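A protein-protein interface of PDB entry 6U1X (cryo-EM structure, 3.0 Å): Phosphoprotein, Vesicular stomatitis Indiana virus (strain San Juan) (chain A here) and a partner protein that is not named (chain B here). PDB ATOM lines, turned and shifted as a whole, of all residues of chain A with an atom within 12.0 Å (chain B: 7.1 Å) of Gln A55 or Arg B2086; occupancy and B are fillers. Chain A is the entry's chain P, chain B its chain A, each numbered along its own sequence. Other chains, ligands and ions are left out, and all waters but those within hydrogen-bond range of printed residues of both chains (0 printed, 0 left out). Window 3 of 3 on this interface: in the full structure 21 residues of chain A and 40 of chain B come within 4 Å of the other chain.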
ATOM      1  N   LYS A  50      -1.631 -27.627  23.121  1.00  0.00           N
ATOM      2  CA  LYS A  50      -3.034 -27.547  22.741  1.00  0.00           C
ATOM      3  C   LYS A  50      -3.584 -26.175  23.115  1.00  0.00           C
ATOM      4  O   LYS A  50      -2.948 -25.448  23.889  1.00  0.00           O
ATOM      5  CB  LYS A  50      -3.834 -28.661  23.419  1.00  0.00           C
ATOM      6  CG  LYS A  50      -3.720 -28.677  24.934  1.00  0.00           C
ATOM      7  CD  LYS A  50      -4.428 -29.876  25.528  1.00  0.00           C
ATOM      8  CE  LYS A  50      -4.174 -29.984  27.019  1.00  0.00           C
ATOM      9  NZ  LYS A  50      -4.767 -31.221  27.590  1.00  0.00           N
ATOM     10  N   PRO A  51      -4.750 -25.777  22.591  1.00  0.00           N
ATOM     11  CA  PRO A  51      -5.274 -24.442  22.909  1.00  0.00           C
ATOM     12  C   PRO A  51      -5.672 -24.288  24.365  1.00  0.00           C
ATOM     13  O   PRO A  51      -5.600 -25.244  25.143  1.00  0.00           O
ATOM     14  CB  PRO A  51      -6.496 -24.315  21.991  1.00  0.00           C
ATOM     15  CG  PRO A  51      -6.357 -25.383  20.981  1.00  0.00           C
ATOM     16  CD  PRO A  51      -5.624 -26.487  21.646  1.00  0.00           C
ATOM     17  N   SER A  52      -6.098 -23.084  24.738  1.00  0.00           N
ATOM     18  CA  SER A  52      -6.584 -22.811  26.090  1.00  0.00           C
ATOM     19  C   SER A  52      -8.092 -23.017  26.192  1.00  0.00           C
ATOM     20  O   SER A  52      -8.841 -22.135  26.607  1.00  0.00           O
ATOM     21  CB  SER A  52      -6.198 -21.395  26.496  1.00  0.00           C
ATOM     22  OG  SER A  52      -4.801 -21.195  26.369  1.00  0.00           O
ATOM     23  N   TYR A  53      -8.544 -24.203  25.796  1.00  0.00           N
ATOM     24  CA  TYR A  53      -9.913 -24.636  26.043  1.00  0.00           C
ATOM     25  C   TYR A  53     -10.003 -26.143  25.847  1.00  0.00           C
ATOM     26  O   TYR A  53      -9.608 -26.663  24.801  1.00  0.00           O
ATOM     27  CB  TYR A  53     -10.898 -23.898  25.137  1.00  0.00           C
ATOM     28  CG  TYR A  53     -10.378 -23.576  23.756  1.00  0.00           C
ATOM     29  CD1 TYR A  53      -9.926 -22.302  23.445  1.00  0.00           C
ATOM     30  CD2 TYR A  53     -10.352 -24.540  22.758  1.00  0.00           C
ATOM     31  CE1 TYR A  53      -9.458 -21.998  22.185  1.00  0.00           C
ATOM     32  CE2 TYR A  53      -9.886 -24.243  21.493  1.00  0.00           C
ATOM     33  CZ  TYR A  53      -9.440 -22.970  21.214  1.00  0.00           C
ATOM     34  OH  TYR A  53      -8.972 -22.671  19.957  1.00  0.00           O
ATOM     35  N   PHE A  54     -10.522 -26.853  26.845  1.00  0.00           N
ATOM     36  CA  PHE A  54     -10.455 -28.306  26.846  1.00  0.00           C
ATOM     37  C   PHE A  54     -11.462 -28.847  27.850  1.00  0.00           C
ATOM     38  O   PHE A  54     -11.561 -28.341  28.970  1.00  0.00           O
ATOM     39  CB  PHE A  54      -9.040 -28.780  27.194  1.00  0.00           C
ATOM     40  CG  PHE A  54      -8.727 -30.169  26.725  1.00  0.00           C
ATOM     41  CD1 PHE A  54      -8.461 -30.415  25.390  1.00  0.00           C
ATOM     42  CD2 PHE A  54      -8.674 -31.224  27.620  1.00  0.00           C
ATOM     43  CE1 PHE A  54      -8.163 -31.689  24.952  1.00  0.00           C
ATOM     44  CE2 PHE A  54      -8.376 -32.501  27.187  1.00  0.00           C
ATOM     45  CZ  PHE A  54      -8.120 -32.734  25.851  1.00  0.00           C
ATOM     46  N   GLN A  55     -12.205 -29.871  27.438  1.00  0.00           N
ATOM     47  CA  GLN A  55     -13.176 -30.508  28.316  1.00  0.00           C
ATOM     48  C   GLN A  55     -12.458 -31.382  29.337  1.00  0.00           C
ATOM     49  O   GLN A  55     -11.542 -32.134  28.988  1.00  0.00           O
ATOM     50  CB  GLN A  55     -14.160 -31.346  27.500  1.00  0.00           C
ATOM     51  CG  GLN A  55     -15.341 -31.901  28.287  1.00  0.00           C
ATOM     52  CD  GLN A  55     -16.304 -30.823  28.751  1.00  0.00           C
ATOM     53  OE1 GLN A  55     -16.107 -29.639  28.482  1.00  0.00           O
ATOM     54  NE2 GLN A  55     -17.355 -31.232  29.451  1.00  0.00           N
ATOM     55  N   ALA A  56     -12.874 -31.282  30.593  1.00  0.00           N
ATOM     56  CA  ALA A  56     -12.298 -32.091  31.659  1.00  0.00           C
ATOM     57  C   ALA A  56     -12.927 -33.479  31.677  1.00  0.00           C
ATOM     58  O   ALA A  56     -14.131 -33.622  31.884  1.00  0.00           O
ATOM     59  CB  ALA A  56     -12.486 -31.411  32.999  1.00  0.00           C
ATOM     60  N   GLN B1987     -12.887 -27.632  10.558  1.00  0.00           N
ATOM     61  CA  GLN B1987     -14.305 -27.699  10.889  1.00  0.00           C
ATOM     62  C   GLN B1987     -15.054 -26.496  10.333  1.00  0.00           C
ATOM     63  O   GLN B1987     -16.165 -26.633   9.806  1.00  0.00           O
ATOM     64  CB  GLN B1987     -14.469 -27.792  12.403  1.00  0.00           C
ATOM     65  CG  GLN B1987     -15.898 -27.809  12.893  1.00  0.00           C
ATOM     66  CD  GLN B1987     -15.992 -28.163  14.361  1.00  0.00           C
ATOM     67  OE1 GLN B1987     -15.446 -29.173  14.802  1.00  0.00           O
ATOM     68  NE2 GLN B1987     -16.678 -27.328  15.128  1.00  0.00           N
ATOM     69  N   SER B2014     -28.384 -26.847  20.609  1.00  0.00           N
ATOM     70  CA  SER B2014     -27.158 -27.634  20.631  1.00  0.00           C
ATOM     71  C   SER B2014     -26.770 -27.929  19.187  1.00  0.00           C
ATOM     72  O   SER B2014     -27.326 -27.348  18.250  1.00  0.00           O
ATOM     73  CB  SER B2014     -27.346 -28.916  21.448  1.00  0.00           C
ATOM     74  OG  SER B2014     -26.169 -29.704  21.429  1.00  0.00           O
ATOM     75  N   THR B2015     -25.801 -28.838  19.006  1.00  0.00           N
ATOM     76  CA  THR B2015     -25.333 -29.189  17.670  1.00  0.00           C
ATOM     77  C   THR B2015     -25.131 -30.691  17.482  1.00  0.00           C
ATOM     78  O   THR B2015     -24.388 -31.092  16.578  1.00  0.00           O
ATOM     79  CB  THR B2015     -24.017 -28.477  17.357  1.00  0.00           C
ATOM     80  OG1 THR B2015     -23.005 -28.922  18.265  1.00  0.00           O
ATOM     81  CG2 THR B2015     -24.182 -26.980  17.483  1.00  0.00           C
ATOM     82  N   ARG B2016     -25.760 -31.530  18.307  1.00  0.00           N
ATOM     83  CA  ARG B2016     -25.678 -32.979  18.155  1.00  0.00           C
ATOM     84  C   ARG B2016     -27.018 -33.691  18.206  1.00  0.00           C
ATOM     85  O   ARG B2016     -27.111 -34.818  17.704  1.00  0.00           O
ATOM     86  CB  ARG B2016     -24.778 -33.584  19.242  1.00  0.00           C
ATOM     87  CG  ARG B2016     -23.340 -33.146  19.172  1.00  0.00           C
ATOM     88  CD  ARG B2016     -22.542 -33.726  20.323  1.00  0.00           C
ATOM     89  NE  ARG B2016     -22.310 -35.157  20.166  1.00  0.00           N
ATOM     90  CZ  ARG B2016     -21.717 -35.928  21.073  1.00  0.00           C
ATOM     91  NH1 ARG B2016     -21.290 -35.418  22.222  1.00  0.00           N
ATOM     92  NH2 ARG B2016     -21.553 -37.221  20.832  1.00  0.00           N
ATOM     93  N   TRP B2070     -19.784 -19.593  31.811  1.00  0.00           N
ATOM     94  CA  TRP B2070     -19.248 -20.716  31.052  1.00  0.00           C
ATOM     95  C   TRP B2070     -19.957 -22.026  31.368  1.00  0.00           C
ATOM     96  O   TRP B2070     -19.956 -22.935  30.530  1.00  0.00           O
ATOM     97  CB  TRP B2070     -17.752 -20.847  31.335  1.00  0.00           C
ATOM     98  CG  TRP B2070     -17.041 -21.873  30.518  1.00  0.00           C
ATOM     99  CD1 TRP B2070     -16.837 -23.180  30.842  1.00  0.00           C
ATOM    100  CD2 TRP B2070     -16.416 -21.674  29.246  1.00  0.00           C
ATOM    101  NE1 TRP B2070     -16.129 -23.810  29.849  1.00  0.00           N
ATOM    102  CE2 TRP B2070     -15.859 -22.906  28.857  1.00  0.00           C
ATOM    103  CE3 TRP B2070     -16.278 -20.574  28.397  1.00  0.00           C
ATOM    104  CZ2 TRP B2070     -15.178 -23.069  27.657  1.00  0.00           C
ATOM    105  CZ3 TRP B2070     -15.602 -20.737  27.207  1.00  0.00           C
ATOM    106  CH2 TRP B2070     -15.058 -21.975  26.847  1.00  0.00           C
ATOM    107  N   ARG B2074     -22.605 -24.518  28.399  1.00  0.00           N
ATOM    108  CA  ARG B2074     -22.121 -25.853  28.079  1.00  0.00           C
ATOM    109  C   ARG B2074     -23.234 -26.879  27.959  1.00  0.00           C
ATOM    110  O   ARG B2074     -23.105 -27.822  27.171  1.00  0.00           O
ATOM    111  CB  ARG B2074     -21.132 -26.322  29.149  1.00  0.00           C
ATOM    112  CG  ARG B2074     -20.348 -27.558  28.771  1.00  0.00           C
ATOM    113  CD  ARG B2074     -19.388 -27.951  29.875  1.00  0.00           C
ATOM    114  NE  ARG B2074     -20.087 -28.425  31.064  1.00  0.00           N
ATOM    115  CZ  ARG B2074     -19.495 -28.727  32.217  1.00  0.00           C
ATOM    116  NH1 ARG B2074     -18.181 -28.606  32.357  1.00  0.00           N
ATOM    117  NH2 ARG B2074     -20.224 -29.151  33.239  1.00  0.00           N
ATOM    118  N   GLY B2078     -24.700 -25.292  23.483  1.00  0.00           N
ATOM    119  CA  GLY B2078     -23.863 -26.024  22.553  1.00  0.00           C
ATOM    120  C   GLY B2078     -22.766 -25.220  21.898  1.00  0.00           C
ATOM    121  O   GLY B2078     -22.242 -25.639  20.863  1.00  0.00           O
ATOM    122  N   ILE B2080     -19.850 -24.392  23.586  1.00  0.00           N
ATOM    123  CA  ILE B2080     -18.692 -25.176  23.996  1.00  0.00           C
ATOM    124  C   ILE B2080     -18.669 -26.496  23.245  1.00  0.00           C
ATOM    125  O   ILE B2080     -17.595 -27.030  22.940  1.00  0.00           O
ATOM    126  CB  ILE B2080     -18.704 -25.405  25.520  1.00  0.00           C
ATOM    127  CG1 ILE B2080     -18.958 -24.096  26.278  1.00  0.00           C
ATOM    128  CG2 ILE B2080     -17.402 -26.042  25.971  1.00  0.00           C
ATOM    129  CD1 ILE B2080     -18.136 -22.939  25.812  1.00  0.00           C
ATOM    130  N   GLU B2081     -19.845 -27.045  22.941  1.00  0.00           N
ATOM    131  CA  GLU B2081     -19.918 -28.246  22.117  1.00  0.00           C
ATOM    132  C   GLU B2081     -19.329 -27.990  20.737  1.00  0.00           C
ATOM    133  O   GLU B2081     -18.702 -28.875  20.144  1.00  0.00           O
ATOM    134  CB  GLU B2081     -21.374 -28.698  22.006  1.00  0.00           C
ATOM    135  CG  GLU B2081     -21.577 -30.196  21.934  1.00  0.00           C
ATOM    136  CD  GLU B2081     -23.043 -30.574  22.009  1.00  0.00           C
ATOM    137  OE1 GLU B2081     -23.880 -29.807  21.491  1.00  0.00           O
ATOM    138  OE2 GLU B2081     -23.361 -31.627  22.599  1.00  0.00           O
ATOM    139  N   TRP B2082     -19.517 -26.778  20.215  1.00  0.00           N
ATOM    140  CA  TRP B2082     -18.937 -26.414  18.929  1.00  0.00           C
ATOM    141  C   TRP B2082     -17.427 -26.256  19.031  1.00  0.00           C
ATOM    142  O   TRP B2082     -16.674 -26.858  18.258  1.00  0.00           O
ATOM    143  CB  TRP B2082     -19.572 -25.120  18.425  1.00  0.00           C
ATOM    144  CG  TRP B2082     -18.757 -24.416  17.394  1.00  0.00           C
ATOM    145  CD1 TRP B2082     -17.847 -23.421  17.603  1.00  0.00           C
ATOM    146  CD2 TRP B2082     -18.777 -24.650  15.987  1.00  0.00           C
ATOM    147  NE1 TRP B2082     -17.297 -23.027  16.412  1.00  0.00           N
ATOM    148  CE2 TRP B2082     -17.854 -23.766  15.403  1.00  0.00           C
ATOM    149  CE3 TRP B2082     -19.488 -25.523  15.163  1.00  0.00           C
ATOM    150  CZ2 TRP B2082     -17.625 -23.730  14.038  1.00  0.00           C
ATOM    151  CZ3 TRP B2082     -19.258 -25.485  13.811  1.00  0.00           C
ATOM    152  CH2 TRP B2082     -18.335 -24.596  13.261  1.00  0.00           C
ATOM    153  N   ILE B2083     -16.971 -25.433  19.977  1.00  0.00           N
ATOM    154  CA  ILE B2083     -15.551 -25.110  20.080  1.00  0.00           C
ATOM    155  C   ILE B2083     -14.726 -26.362  20.339  1.00  0.00           C
ATOM    156  O   ILE B2083     -13.593 -26.479  19.856  1.00  0.00           O
ATOM    157  CB  ILE B2083     -15.325 -24.054  21.177  1.00  0.00           C
ATOM    158  CG1 ILE B2083     -16.015 -22.739  20.801  1.00  0.00           C
ATOM    159  CG2 ILE B2083     -13.836 -23.842  21.401  1.00  0.00           C
ATOM    160  CD1 ILE B2083     -16.126 -21.753  21.938  1.00  0.00           C
ATOM    161  N   ASN B2084     -15.271 -27.312  21.093  1.00  0.00           N
ATOM    162  CA  ASN B2084     -14.557 -28.520  21.477  1.00  0.00           C
ATOM    163  C   ASN B2084     -14.714 -29.648  20.461  1.00  0.00           C
ATOM    164  O   ASN B2084     -14.474 -30.812  20.799  1.00  0.00           O
ATOM    165  CB  ASN B2084     -15.015 -28.975  22.862  1.00  0.00           C
ATOM    166  CG  ASN B2084     -14.691 -27.957  23.939  1.00  0.00           C
ATOM    167  OD1 ASN B2084     -14.541 -26.767  23.659  1.00  0.00           O
ATOM    168  ND2 ASN B2084     -14.574 -28.421  25.176  1.00  0.00           N
ATOM    169  N   ARG B2085     -15.095 -29.324  19.225  1.00  0.00           N
ATOM    170  CA  ARG B2085     -15.117 -30.283  18.121  1.00  0.00           C
ATOM    171  C   ARG B2085     -16.052 -31.460  18.405  1.00  0.00           C
ATOM    172  O   ARG B2085     -15.645 -32.624  18.439  1.00  0.00           O
ATOM    173  CB  ARG B2085     -13.702 -30.779  17.819  1.00  0.00           C
ATOM    174  CG  ARG B2085     -12.704 -29.679  17.525  1.00  0.00           C
ATOM    175  CD  ARG B2085     -11.322 -30.240  17.266  1.00  0.00           C
ATOM    176  NE  ARG B2085     -11.276 -31.060  16.056  1.00  0.00           N
ATOM    177  CZ  ARG B2085     -11.450 -32.379  16.005  1.00  0.00           C
ATOM    178  NH1 ARG B2085     -11.699 -33.088  17.100  1.00  0.00           N
ATOM    179  NH2 ARG B2085     -11.382 -33.000  14.836  1.00  0.00           N
ATOM    180  N   ARG B2086     -17.326 -31.131  18.605  1.00  0.00           N
ATOM    181  CA  ARG B2086     -18.372 -32.145  18.739  1.00  0.00           C
ATOM    182  C   ARG B2086     -19.639 -31.555  18.128  1.00  0.00           C
ATOM    183  O   ARG B2086     -20.301 -30.717  18.748  1.00  0.00           O
ATOM    184  CB  ARG B2086     -18.577 -32.540  20.195  1.00  0.00           C
ATOM    185  CG  ARG B2086     -17.441 -33.367  20.768  1.00  0.00           C
ATOM    186  CD  ARG B2086     -17.721 -33.802  22.191  1.00  0.00           C
ATOM    187  NE  ARG B2086     -17.647 -32.685  23.131  1.00  0.00           N
ATOM    188  CZ  ARG B2086     -16.518 -32.193  23.633  1.00  0.00           C
ATOM    189  NH1 ARG B2086     -15.339 -32.700  23.292  1.00  0.00           N
ATOM    190  NH2 ARG B2086     -16.566 -31.178  24.482  1.00  0.00           N
ATOM    191  N   ILE B2087     -19.963 -31.995  16.913  1.00  0.00           N
ATOM    192  CA  ILE B2087     -21.030 -31.424  16.105  1.00  0.00           C
ATOM    193  C   ILE B2087     -21.761 -32.549  15.382  1.00  0.00           C
ATOM    194  O   ILE B2087     -21.394 -33.723  15.475  1.00  0.00           O
ATOM    195  CB  ILE B2087     -20.495 -30.388  15.095  1.00  0.00           C
ATOM    196  CG1 ILE B2087     -19.379 -30.997  14.238  1.00  0.00           C
ATOM    197  CG2 ILE B2087     -19.991 -29.170  15.826  1.00  0.00           C
ATOM    198  CD1 ILE B2087     -18.906 -30.099  13.123  1.00  0.00           C
ATOM    199  N   SER B2088     -22.804 -32.173  14.647  1.00  0.00           N
ATOM    200  CA  SER B2088     -23.568 -33.103  13.828  1.00  0.00           C
ATOM    201  C   SER B2088     -23.007 -33.116  12.414  1.00  0.00           C
ATOM    202  O   SER B2088     -22.905 -32.067  11.769  1.00  0.00           O
ATOM    203  CB  SER B2088     -25.043 -32.703  13.805  1.00  0.00           C
ATOM    204  OG  SER B2088     -25.809 -33.595  13.016  1.00  0.00           O
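Of the 7 printed residues of chain A, 2 touch a printed residue of chain B. Of the 16 printed residues of chain B, 4 touch a printed residue of chain A. Hydrophobic or aromatic side chains of chain B that line the printed part of chain A: Ile B2083. Among the printed residues, 4 pairs touch across the chains.
Gln A55 touches just these residues of chain B: Arg B2074, Asn B2084 and Arg B2086. Of chain A, only Gln A55 (3.9 Å) comes within 4 Å of Arg B2086. No residue of chain A comes within 4 Å of Thr B2015. No residue of chain A comes within 4 Å of Ile B2080. No residue of chain A comes within 4 Å of Glu B2081. Of chain A, only Gln A55 comes within 4 Å of Asn B2084. No residue of chain A comes within 4 Å of Arg B2085. No residue of chain A comes within 4 Å of Ile B2087. Printed residues of chain B within 4 Å of Tyr A53: Ile B2083 (3.8 Å). Printed residues of chain A within 4 Å of Ile B2083: Tyr A53 (3.8 Å). Arg B2016 touches none of the printed residues of chain A. The nearest printed residue of chain A that does not touch Ile B2083 is Phe A54 (7.0 Å).
Among the printed residues, pairs that only touch across the chains: Tyr A53 with Ile B2083 (3.8 Å), Gln A55 with Arg B2074 (3.9 Å), Gln A55 with Asn B2084 (3.6 Å) and Gln A55 with Arg B2086 (3.9 Å).
The backbone carbonyl oxygen (O) of Ile B2080 lies close to the side-chain amide oxygen (OD1) of Asn B2084, at 3.1 Å. The backbone carbonyl oxygen of Asn B2084 lies within hydrogen-bond range of the guanidinium group of Arg B2086 (3.2 Å). The side-chain hydroxyl (OG1) of Thr B2015 lies within hydrogen-bond range of the backbone carbonyl oxygen (O) of Arg B2086, 3.3 Å away. The backbone carbonyl oxygen of Glu B2081 is in hydrogen-bond range of the backbone NH of Arg B2086, at 3.1 Å.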
